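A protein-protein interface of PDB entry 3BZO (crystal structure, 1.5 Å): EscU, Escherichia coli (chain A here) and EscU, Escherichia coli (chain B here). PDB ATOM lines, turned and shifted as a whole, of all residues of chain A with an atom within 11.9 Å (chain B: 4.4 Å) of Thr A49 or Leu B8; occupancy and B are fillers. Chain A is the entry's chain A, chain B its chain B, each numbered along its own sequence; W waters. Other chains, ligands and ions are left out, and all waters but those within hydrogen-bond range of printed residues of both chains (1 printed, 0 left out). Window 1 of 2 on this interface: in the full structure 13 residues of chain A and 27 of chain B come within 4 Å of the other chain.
Of the 14 printed residues of chain A, 8 touch a printed residue of chain B.
Printed residues of chain A that touch a printed residue of chain B: Ile A45, Lys A46, Lys A47, Ser A48, Thr A49, Val A50, Ile A51 and Val A52.
Printed residues of chain B that touch a printed residue of chain A: Ile B6, Cys B7, Leu B8, Tyr B9, Tyr B10, Ile B41, Pro B42, Leu B74 and Ala B78.
Among the printed residues, no Asp or Glu carboxylate lies within 4 Å of a Lys or Arg side-chain nitrogen of the other chain.
Water W1 bridges the backbone carbonyl oxygen (O) of Thr A49 (2.7 Å) and the backbone carbonyl oxygen (O) of Ala B78 (2.8 Å).
Ile A45 touches Cys B7.
CD1 of Ile B41 touches O of Ile A45, 3.4 Å away.
Lys A46 touches Ile B41.
Leu B8 touches Ser A48.
CB of Ala B78 touches O of Thr A49, 3.7 Å away.
Val A50 touches Cys B7.
CA of Val A50 touches O of Pro B42 (3.6 Å).
CD1 of Ile A51 touches SG of Cys B7, 3.7 Å away.
CD1 of Leu B8 touches CG2 of Val A52 (3.9 Å).
Val A52 touches Leu B74.
O of Val A50 is in hydrogen-bond range of N of Leu B8, at 2.9 Å.
N of Ile A51 is in hydrogen-bond range of O of Pro B42 (2.9 Å).
N of Thr A49 lies within hydrogen-bond range of O of Leu B8 (2.9 Å).
The backbone carbonyl oxygen of Ile B6 is in hydrogen-bond range of the backbone NH of Val A52.
The side-chain sulfur of Cys B7 sits close to the side-chain hydroxyl of Ser A48.
OG1 of Thr A49 sits at hydrogen-bond distance from N of Tyr B10 (3.0 Å).
The side-chain hydroxyl (OG) of Ser A48 sits at hydrogen-bond distance from the backbone carbonyl oxygen (O) of Ile A45.
N of Tyr B9 lies within hydrogen-bond range of O of Leu B19, 2.8 Å away.
Of the printed residues of chain B, Ile A45 touches Cys B7 and Ile B41.
Printed residues of chain B within 4 Å of Lys A47: Tyr B9 (3.3 Å).
Of the printed residues of chain B, Ser A48 touches Cys B7 (3.0 Å), Leu B8 (3.7 Å) and Ile B41 (3.4 Å).
Thr A49 touches just these residues of chain B: Leu B8, Tyr B9, Tyr B10, Pro B42 and Ala B78.
Of the printed residues of chain B, Val A50 touches Ile B6 (3.9 Å), Cys B7 (3.8 Å), Leu B8 (2.9 Å), Pro B42 (3.6 Å) and Ala B78 (3.7 Å).
Printed residues of chain B within 4 Å of Val A52: Ile B6 (2.8 Å), Leu B8 (3.9 Å) and Leu B74 (3.2 Å).
Ile B6 touches just these residues of chain A: Val A50, Ile A51 and Val A52.
Of the printed residues of chain A, Leu B8 touches Ser A48, Thr A49, Val A50 and Val A52.
Tyr B9 touches just these residues of chain A: Lys A47 (3.3 Å) and Thr A49 (3.6 Å).
No residue of chain A comes within 4 Å of Val B20.
Pro B42 touches three residues of chain A.
Ile B63 touches none of the printed residues of chain A.
No residue of chain A comes within 4 Å of Val B71.
Leu B74 touches just one residue of chain A: Val A52 (3.2 Å).
Of chain A, only Thr A49 (3.7 Å) and Val A50 (3.7 Å) come within 4 Å of Ala B78.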
ATOM      1  N   LEU A  41     -15.985  -2.127   7.941  1.00  0.00           N
ATOM      2  CA  LEU A  41     -17.186  -2.189   7.123  1.00  0.00           C
ATOM      3  C   LEU A  41     -18.359  -1.630   7.899  1.00  0.00           C
ATOM      4  O   LEU A  41     -19.056  -0.752   7.418  1.00  0.00           O
ATOM      5  CB  LEU A  41     -17.502  -3.617   6.675  1.00  0.00           C
ATOM      6  CG  LEU A  41     -18.823  -3.821   5.933  1.00  0.00           C
ATOM      7  CD1 LEU A  41     -18.836  -2.982   4.659  1.00  0.00           C
ATOM      8  CD2 LEU A  41     -19.074  -5.312   5.646  1.00  0.00           C
ATOM      9  N   ALA A  42     -18.560  -2.138   9.114  1.00  0.00           N
ATOM     10  CA  ALA A  42     -19.721  -1.712   9.895  1.00  0.00           C
ATOM     11  C   ALA A  42     -19.674  -0.221  10.219  1.00  0.00           C
ATOM     12  O   ALA A  42     -20.700   0.444  10.180  1.00  0.00           O
ATOM     13  CB  ALA A  42     -19.881  -2.545  11.152  1.00  0.00           C
ATOM     14  N   ASN A  43     -18.493   0.301  10.553  1.00  0.00           N
ATOM     15  CA  ASN A  43     -18.361   1.729  10.873  1.00  0.00           C
ATOM     16  C   ASN A  43     -18.600   2.601   9.647  1.00  0.00           C
ATOM     17  O   ASN A  43     -19.194   3.677   9.736  1.00  0.00           O
ATOM     18  CB  ASN A  43     -16.982   2.041  11.477  1.00  0.00           C
ATOM     19  CG  ASN A  43     -16.832   1.505  12.882  1.00  0.00           C
ATOM     20  OD1 ASN A  43     -17.808   1.401  13.627  1.00  0.00           O
ATOM     21  ND2 ASN A  43     -15.615   1.175  13.256  1.00  0.00           N
ATOM     22  N   ASN A  44     -18.165   2.129   8.496  1.00  0.00           N
ATOM     23  CA  ASN A  44     -18.501   2.854   7.268  1.00  0.00           C
ATOM     24  C   ASN A  44     -20.004   2.885   6.989  1.00  0.00           C
ATOM     25  O   ASN A  44     -20.562   3.952   6.659  1.00  0.00           O
ATOM     26  CB  ASN A  44     -17.735   2.278   6.077  1.00  0.00           C
ATOM     27  CG  ASN A  44     -16.287   2.742   6.043  1.00  0.00           C
ATOM     28  OD1 ASN A  44     -15.935   3.768   6.625  1.00  0.00           O
ATOM     29  ND2 ASN A  44     -15.445   1.993   5.354  1.00  0.00           N
ATOM     30  N   ILE A  45     -20.670   1.744   7.113  1.00  0.00           N
ATOM     31  CA  ILE A  45     -22.101   1.717   6.891  1.00  0.00           C
ATOM     32  C   ILE A  45     -22.795   2.610   7.917  1.00  0.00           C
ATOM     33  O   ILE A  45     -23.667   3.364   7.568  1.00  0.00           O
ATOM     34  CB  ILE A  45     -22.728   0.303   6.920  1.00  0.00           C
ATOM     35  CG1 ILE A  45     -22.063  -0.636   5.900  1.00  0.00           C
ATOM     36  CG2 ILE A  45     -24.254   0.413   6.666  1.00  0.00           C
ATOM     37  CD1 ILE A  45     -22.206  -0.215   4.470  1.00  0.00           C
ATOM     38  N   LYS A  46     -22.385   2.542   9.183  1.00  0.00           N
ATOM     39  CA  LYS A  46     -23.061   3.334  10.213  1.00  0.00           C
ATOM     40  C   LYS A  46     -23.072   4.833   9.893  1.00  0.00           C
ATOM     41  O   LYS A  46     -24.065   5.514  10.144  1.00  0.00           O
ATOM     42  CB  LYS A  46     -22.426   3.079  11.587  1.00  0.00           C
ATOM     43  CG  LYS A  46     -23.103   3.829  12.737  1.00  0.00           C
ATOM     44  CD  LYS A  46     -22.627   3.318  14.081  1.00  0.00           C
ATOM     45  CE  LYS A  46     -23.122   4.175  15.241  1.00  0.00           C
ATOM     46  NZ  LYS A  46     -22.544   3.689  16.530  1.00  0.00           N
ATOM     47  N   LYS A  47     -21.991   5.336   9.317  1.00  0.00           N
ATOM     48  CA  LYS A  47     -21.899   6.774   9.048  1.00  0.00           C
ATOM     49  C   LYS A  47     -22.422   7.161   7.669  1.00  0.00           C
ATOM     50  O   LYS A  47     -22.514   8.358   7.358  1.00  0.00           O
ATOM     51  CB  LYS A  47     -20.462   7.266   9.202  1.00  0.00           C
ATOM     52  CG  LYS A  47     -19.529   6.869   8.073  1.00  0.00           C
ATOM     53  CD  LYS A  47     -18.169   7.504   8.266  1.00  0.00           C
ATOM     54  CE  LYS A  47     -17.392   7.537   6.984  1.00  0.00           C
ATOM     55  NZ  LYS A  47     -16.005   8.012   7.222  1.00  0.00           N
ATOM     56  N   SER A  48     -22.756   6.181   6.841  1.00  0.00           N
ATOM     57  CA  SER A  48     -23.095   6.474   5.453  1.00  0.00           C
ATOM     58  C   SER A  48     -24.433   7.178   5.312  1.00  0.00           C
ATOM     59  O   SER A  48     -25.264   7.184   6.229  1.00  0.00           O
ATOM     60  CB  SER A  48     -23.108   5.193   4.629  1.00  0.00           C
ATOM     61  OG  SER A  48     -24.190   4.362   5.014  1.00  0.00           O
ATOM     62  N   THR A  49     -24.635   7.747   4.127  1.00  0.00           N
ATOM     63  CA  THR A  49     -25.784   8.591   3.831  1.00  0.00           C
ATOM     64  C   THR A  49     -26.915   7.804   3.159  1.00  0.00           C
ATOM     65  O   THR A  49     -28.099   7.943   3.490  1.00  0.00           O
ATOM     66  CB  THR A  49     -25.339   9.785   2.936  1.00  0.00           C
ATOM     67  OG1 THR A  49     -24.234  10.447   3.572  1.00  0.00           O
ATOM     68  CG2 THR A  49     -26.492  10.770   2.682  1.00  0.00           C
ATOM     69  N   VAL A  50     -26.564   6.977   2.191  1.00  0.00           N
ATOM     70  CA  VAL A  50     -27.567   6.210   1.477  1.00  0.00           C
ATOM     71  C   VAL A  50     -26.910   5.028   0.792  1.00  0.00           C
ATOM     72  O   VAL A  50     -25.755   5.123   0.404  1.00  0.00           O
ATOM     73  CB  VAL A  50     -28.284   7.099   0.444  1.00  0.00           C
ATOM     74  CG1 VAL A  50     -27.277   7.626  -0.600  1.00  0.00           C
ATOM     75  CG2 VAL A  50     -29.454   6.357  -0.199  1.00  0.00           C
ATOM     76  N   ILE A  51     -27.651   3.919   0.686  1.00  0.00           N
ATOM     77  CA  ILE A  51     -27.201   2.729  -0.020  1.00  0.00           C
ATOM     78  C   ILE A  51     -28.041   2.606  -1.276  1.00  0.00           C
ATOM     79  O   ILE A  51     -29.262   2.714  -1.200  1.00  0.00           O
ATOM     80  CB  ILE A  51     -27.463   1.440   0.784  1.00  0.00           C
ATOM     81  CG1 ILE A  51     -26.890   1.528   2.192  1.00  0.00           C
ATOM     82  CG2 ILE A  51     -26.957   0.201   0.030  1.00  0.00           C
ATOM     83  CD1 ILE A  51     -25.512   1.949   2.226  1.00  0.00           C
ATOM     84  N   VAL A  52     -27.401   2.397  -2.415  1.00  0.00           N
ATOM     85  CA  VAL A  52     -28.110   2.074  -3.658  1.00  0.00           C
ATOM     86  C   VAL A  52     -27.868   0.608  -3.958  1.00  0.00           C
ATOM     87  O   VAL A  52     -26.730   0.147  -3.940  1.00  0.00           O
ATOM     88  CB  VAL A  52     -27.621   2.915  -4.850  1.00  0.00           C
ATOM     89  CG1 VAL A  52     -28.596   2.784  -6.022  1.00  0.00           C
ATOM     90  CG2 VAL A  52     -27.513   4.347  -4.458  1.00  0.00           C
ATOM     91  N   LYS A  53     -28.947  -0.107  -4.269  1.00  0.00           N
ATOM     92  CA  LYS A  53     -28.861  -1.523  -4.556  1.00  0.00           C
ATOM     93  C   LYS A  53     -29.596  -1.835  -5.846  1.00  0.00           C
ATOM     94  O   LYS A  53     -30.410  -1.033  -6.316  1.00  0.00           O
ATOM     95  CB  LYS A  53     -29.432  -2.369  -3.413  1.00  0.00           C
ATOM     96  CG  LYS A  53     -30.945  -2.251  -3.201  1.00  0.00           C
ATOM     97  CD  LYS A  53     -31.447  -3.149  -2.045  1.00  0.00           C
ATOM     98  CE  LYS A  53     -31.483  -4.628  -2.444  1.00  0.00           C
ATOM     99  NZ  LYS A  53     -32.518  -4.914  -3.499  1.00  0.00           N
ATOM    100  N   ASN A  54     -29.266  -2.982  -6.428  1.00  0.00           N
ATOM    101  CA  ASN A  54     -30.020  -3.516  -7.546  1.00  0.00           C
ATOM    102  C   ASN A  54     -31.043  -4.506  -7.017  1.00  0.00           C
ATOM    103  O   ASN A  54     -31.358  -4.476  -5.831  1.00  0.00           O
ATOM    104  CB  ASN A  54     -29.101  -4.166  -8.583  1.00  0.00           C
ATOM    105  CG  ASN A  54     -28.469  -5.442  -8.092  1.00  0.00           C
ATOM    106  OD1 ASN A  54     -28.432  -5.711  -6.886  1.00  0.00           O
ATOM    107  ND2 ASN A  54     -27.912  -6.216  -9.015  1.00  0.00           N
ATOM    108  OXT ASN A  54     -31.554  -5.367  -7.731  1.00  0.00           O
ATOM    109  N   ILE B   6     -24.040  -0.289  -3.099  1.00  0.00           N
ATOM    110  CA  ILE B   6     -23.132   0.841  -3.161  1.00  0.00           C
ATOM    111  C   ILE B   6     -23.469   1.765  -2.020  1.00  0.00           C
ATOM    112  O   ILE B   6     -24.603   2.238  -1.903  1.00  0.00           O
ATOM    113  CB  ILE B   6     -23.343   1.658  -4.451  1.00  0.00           C
ATOM    114  CG1 ILE B   6     -23.327   0.761  -5.696  1.00  0.00           C
ATOM    115  CG2 ILE B   6     -22.300   2.768  -4.556  1.00  0.00           C
ATOM    116  CD1 ILE B   6     -22.041   0.159  -5.966  1.00  0.00           C
ATOM    117  N   CYS B   7     -22.476   2.022  -1.180  1.00  0.00           N
ATOM    118  CA  CYS B   7     -22.652   2.850   0.005  1.00  0.00           C
ATOM    119  C   CYS B   7     -22.080   4.233  -0.271  1.00  0.00           C
ATOM    120  O   CYS B   7     -20.871   4.370  -0.474  1.00  0.00           O
ATOM    121  CB  CYS B   7     -21.917   2.221   1.193  1.00  0.00           C
ATOM    122  SG  CYS B   7     -22.037   3.148   2.731  1.00  0.00           S
ATOM    123  N   LEU B   8     -22.948   5.240  -0.260  1.00  0.00           N
ATOM    124  CA  LEU B   8     -22.558   6.616  -0.528  1.00  0.00           C
ATOM    125  C   LEU B   8     -22.503   7.422   0.754  1.00  0.00           C
ATOM    126  O   LEU B   8     -23.397   7.313   1.592  1.00  0.00           O
ATOM    127  CB  LEU B   8     -23.573   7.264  -1.456  1.00  0.00           C
ATOM    128  CG  LEU B   8     -23.451   6.791  -2.901  1.00  0.00           C
ATOM    129  CD1 LEU B   8     -24.793   6.930  -3.561  1.00  0.00           C
ATOM    130  CD2 LEU B   8     -22.375   7.553  -3.675  1.00  0.00           C
ATOM    131  N   TYR B   9     -21.474   8.251   0.859  1.00  0.00           N
ATOM    132  CA  TYR B   9     -21.257   9.110   2.012  1.00  0.00           C
ATOM    133  C   TYR B   9     -21.089  10.545   1.525  1.00  0.00           C
ATOM    134  O   TYR B   9     -20.260  10.831   0.672  1.00  0.00           O
ATOM    135  CB  TYR B   9     -20.013   8.648   2.770  1.00  0.00           C
ATOM    136  CG  TYR B   9     -19.650   9.508   3.952  1.00  0.00           C
ATOM    137  CD1 TYR B   9     -18.428  10.146   4.009  1.00  0.00           C
ATOM    138  CD2 TYR B   9     -20.529   9.676   5.011  1.00  0.00           C
ATOM    139  CE1 TYR B   9     -18.079  10.920   5.096  1.00  0.00           C
ATOM    140  CE2 TYR B   9     -20.196  10.453   6.100  1.00  0.00           C
ATOM    141  CZ  TYR B   9     -18.972  11.076   6.142  1.00  0.00           C
ATOM    142  OH  TYR B   9     -18.638  11.856   7.240  1.00  0.00           O
ATOM    143  N   TYR B  10     -21.893  11.448   2.062  1.00  0.00           N
ATOM    144  CA  TYR B  10     -21.684  12.858   1.796  1.00  0.00           C
ATOM    145  C   TYR B  10     -21.902  13.655   3.069  1.00  0.00           C
ATOM    146  O   TYR B  10     -22.932  13.542   3.725  1.00  0.00           O
ATOM    147  CB  TYR B  10     -22.611  13.356   0.707  1.00  0.00           C
ATOM    148  CG  TYR B  10     -22.342  14.798   0.303  1.00  0.00           C
ATOM    149  CD1 TYR B  10     -23.286  15.790   0.517  1.00  0.00           C
ATOM    150  CD2 TYR B  10     -21.125  15.159  -0.248  1.00  0.00           C
ATOM    151  CE1 TYR B  10     -23.034  17.103   0.160  1.00  0.00           C
ATOM    152  CE2 TYR B  10     -20.858  16.475  -0.607  1.00  0.00           C
ATOM    153  CZ  TYR B  10     -21.818  17.443  -0.416  1.00  0.00           C
ATOM    154  OH  TYR B  10     -21.541  18.753  -0.769  1.00  0.00           O
ATOM    155  N   LEU B  19     -19.040  10.366  -1.909  1.00  0.00           N
ATOM    156  CA  LEU B  19     -17.963   9.386  -1.904  1.00  0.00           C
ATOM    157  C   LEU B  19     -18.572   7.997  -1.833  1.00  0.00           C
ATOM    158  O   LEU B  19     -19.485   7.767  -1.037  1.00  0.00           O
ATOM    159  CB  LEU B  19     -17.104   9.599  -0.652  1.00  0.00           C
ATOM    160  CG  LEU B  19     -15.847   8.753  -0.425  1.00  0.00           C
ATOM    161  CD1 LEU B  19     -14.828   8.920  -1.522  1.00  0.00           C
ATOM    162  CD2 LEU B  19     -15.232   9.105   0.911  1.00  0.00           C
ATOM    163  N   VAL B  20     -18.053   7.073  -2.645  1.00  0.00           N
ATOM    164  CA  VAL B  20     -18.408   5.666  -2.516  1.00  0.00           C
ATOM    165  C   VAL B  20     -17.435   5.106  -1.508  1.00  0.00           C
ATOM    166  O   VAL B  20     -16.241   4.908  -1.794  1.00  0.00           O
ATOM    167  CB  VAL B  20     -18.303   4.922  -3.833  1.00  0.00           C
ATOM    168  CG1 VAL B  20     -18.425   3.435  -3.613  1.00  0.00           C
ATOM    169  CG2 VAL B  20     -19.392   5.402  -4.812  1.00  0.00           C
ATOM    170  N   ILE B  41     -29.948   3.051   7.787  1.00  0.00           N
ATOM    171  CA  ILE B  41     -29.463   3.822   6.631  1.00  0.00           C
ATOM    172  C   ILE B  41     -30.449   3.607   5.491  1.00  0.00           C
ATOM    173  O   ILE B  41     -30.775   2.459   5.178  1.00  0.00           O
ATOM    174  CB  ILE B  41     -28.088   3.346   6.158  1.00  0.00           C
ATOM    175  CG1 ILE B  41     -27.104   3.234   7.334  1.00  0.00           C
ATOM    176  CG2 ILE B  41     -27.543   4.251   5.029  1.00  0.00           C
ATOM    177  CD1 ILE B  41     -26.819   4.536   8.045  1.00  0.00           C
ATOM    178  N   PRO B  42     -30.955   4.697   4.880  1.00  0.00           N
ATOM    179  CA  PRO B  42     -31.873   4.505   3.763  1.00  0.00           C
ATOM    180  C   PRO B  42     -31.273   3.645   2.642  1.00  0.00           C
ATOM    181  O   PRO B  42     -30.120   3.854   2.268  1.00  0.00           O
ATOM    182  CB  PRO B  42     -32.126   5.933   3.271  1.00  0.00           C
ATOM    183  CG  PRO B  42     -31.948   6.787   4.522  1.00  0.00           C
ATOM    184  CD  PRO B  42     -30.780   6.127   5.219  1.00  0.00           C
ATOM    185  N   ILE B  63     -17.801  10.291  -6.708  1.00  0.00           N
ATOM    186  CA  ILE B  63     -18.604  10.158  -7.913  1.00  0.00           C
ATOM    187  C   ILE B  63     -18.119  11.159  -8.961  1.00  0.00           C
ATOM    188  O   ILE B  63     -17.480  12.191  -8.664  1.00  0.00           O
ATOM    189  CB  ILE B  63     -20.102  10.335  -7.643  1.00  0.00           C
ATOM    190  CG1 ILE B  63     -20.410  11.765  -7.169  1.00  0.00           C
ATOM    191  CG2 ILE B  63     -20.590   9.284  -6.634  1.00  0.00           C
ATOM    192  CD1 ILE B  63     -21.907  12.072  -7.146  1.00  0.00           C
ATOM    193  N   VAL B  71     -27.275  11.111  -8.015  1.00  0.00           N
ATOM    194  CA  VAL B  71     -26.910  10.922  -6.627  1.00  0.00           C
ATOM    195  C   VAL B  71     -27.455  12.062  -5.756  1.00  0.00           C
ATOM    196  O   VAL B  71     -27.851  11.824  -4.621  1.00  0.00           O
ATOM    197  CB  VAL B  71     -25.395  10.766  -6.448  1.00  0.00           C
ATOM    198  CG1 VAL B  71     -25.009  10.888  -4.975  1.00  0.00           C
ATOM    199  CG2 VAL B  71     -24.931   9.423  -7.047  1.00  0.00           C
ATOM    200  N   LEU B  74     -30.857  11.164  -4.693  1.00  0.00           N
ATOM    201  CA  LEU B  74     -30.821  10.162  -3.604  1.00  0.00           C
ATOM    202  C   LEU B  74     -30.547  10.850  -2.281  1.00  0.00           C
ATOM    203  O   LEU B  74     -31.157  10.550  -1.264  1.00  0.00           O
ATOM    204  CB  LEU B  74     -29.709   9.124  -3.816  1.00  0.00           C
ATOM    205  CG  LEU B  74     -29.792   8.090  -4.937  1.00  0.00           C
ATOM    206  CD1 LEU B  74     -28.476   7.344  -5.082  1.00  0.00           C
ATOM    207  CD2 LEU B  74     -30.888   7.110  -4.659  1.00  0.00           C
ATOM    208  N   ALA B  78     -32.721  10.913   1.186  1.00  0.00           N
ATOM    209  CA  ALA B  78     -32.145  10.095   2.251  1.00  0.00           C
ATOM    210  C   ALA B  78     -31.642  10.927   3.421  1.00  0.00           C
ATOM    211  O   ALA B  78     -31.514  10.416   4.534  1.00  0.00           O
ATOM    212  CB  ALA B  78     -31.000   9.250   1.695  1.00  0.00           C
HETATM  213  O   HOH W   1     -29.151   9.321   5.585  1.00  0.00           O
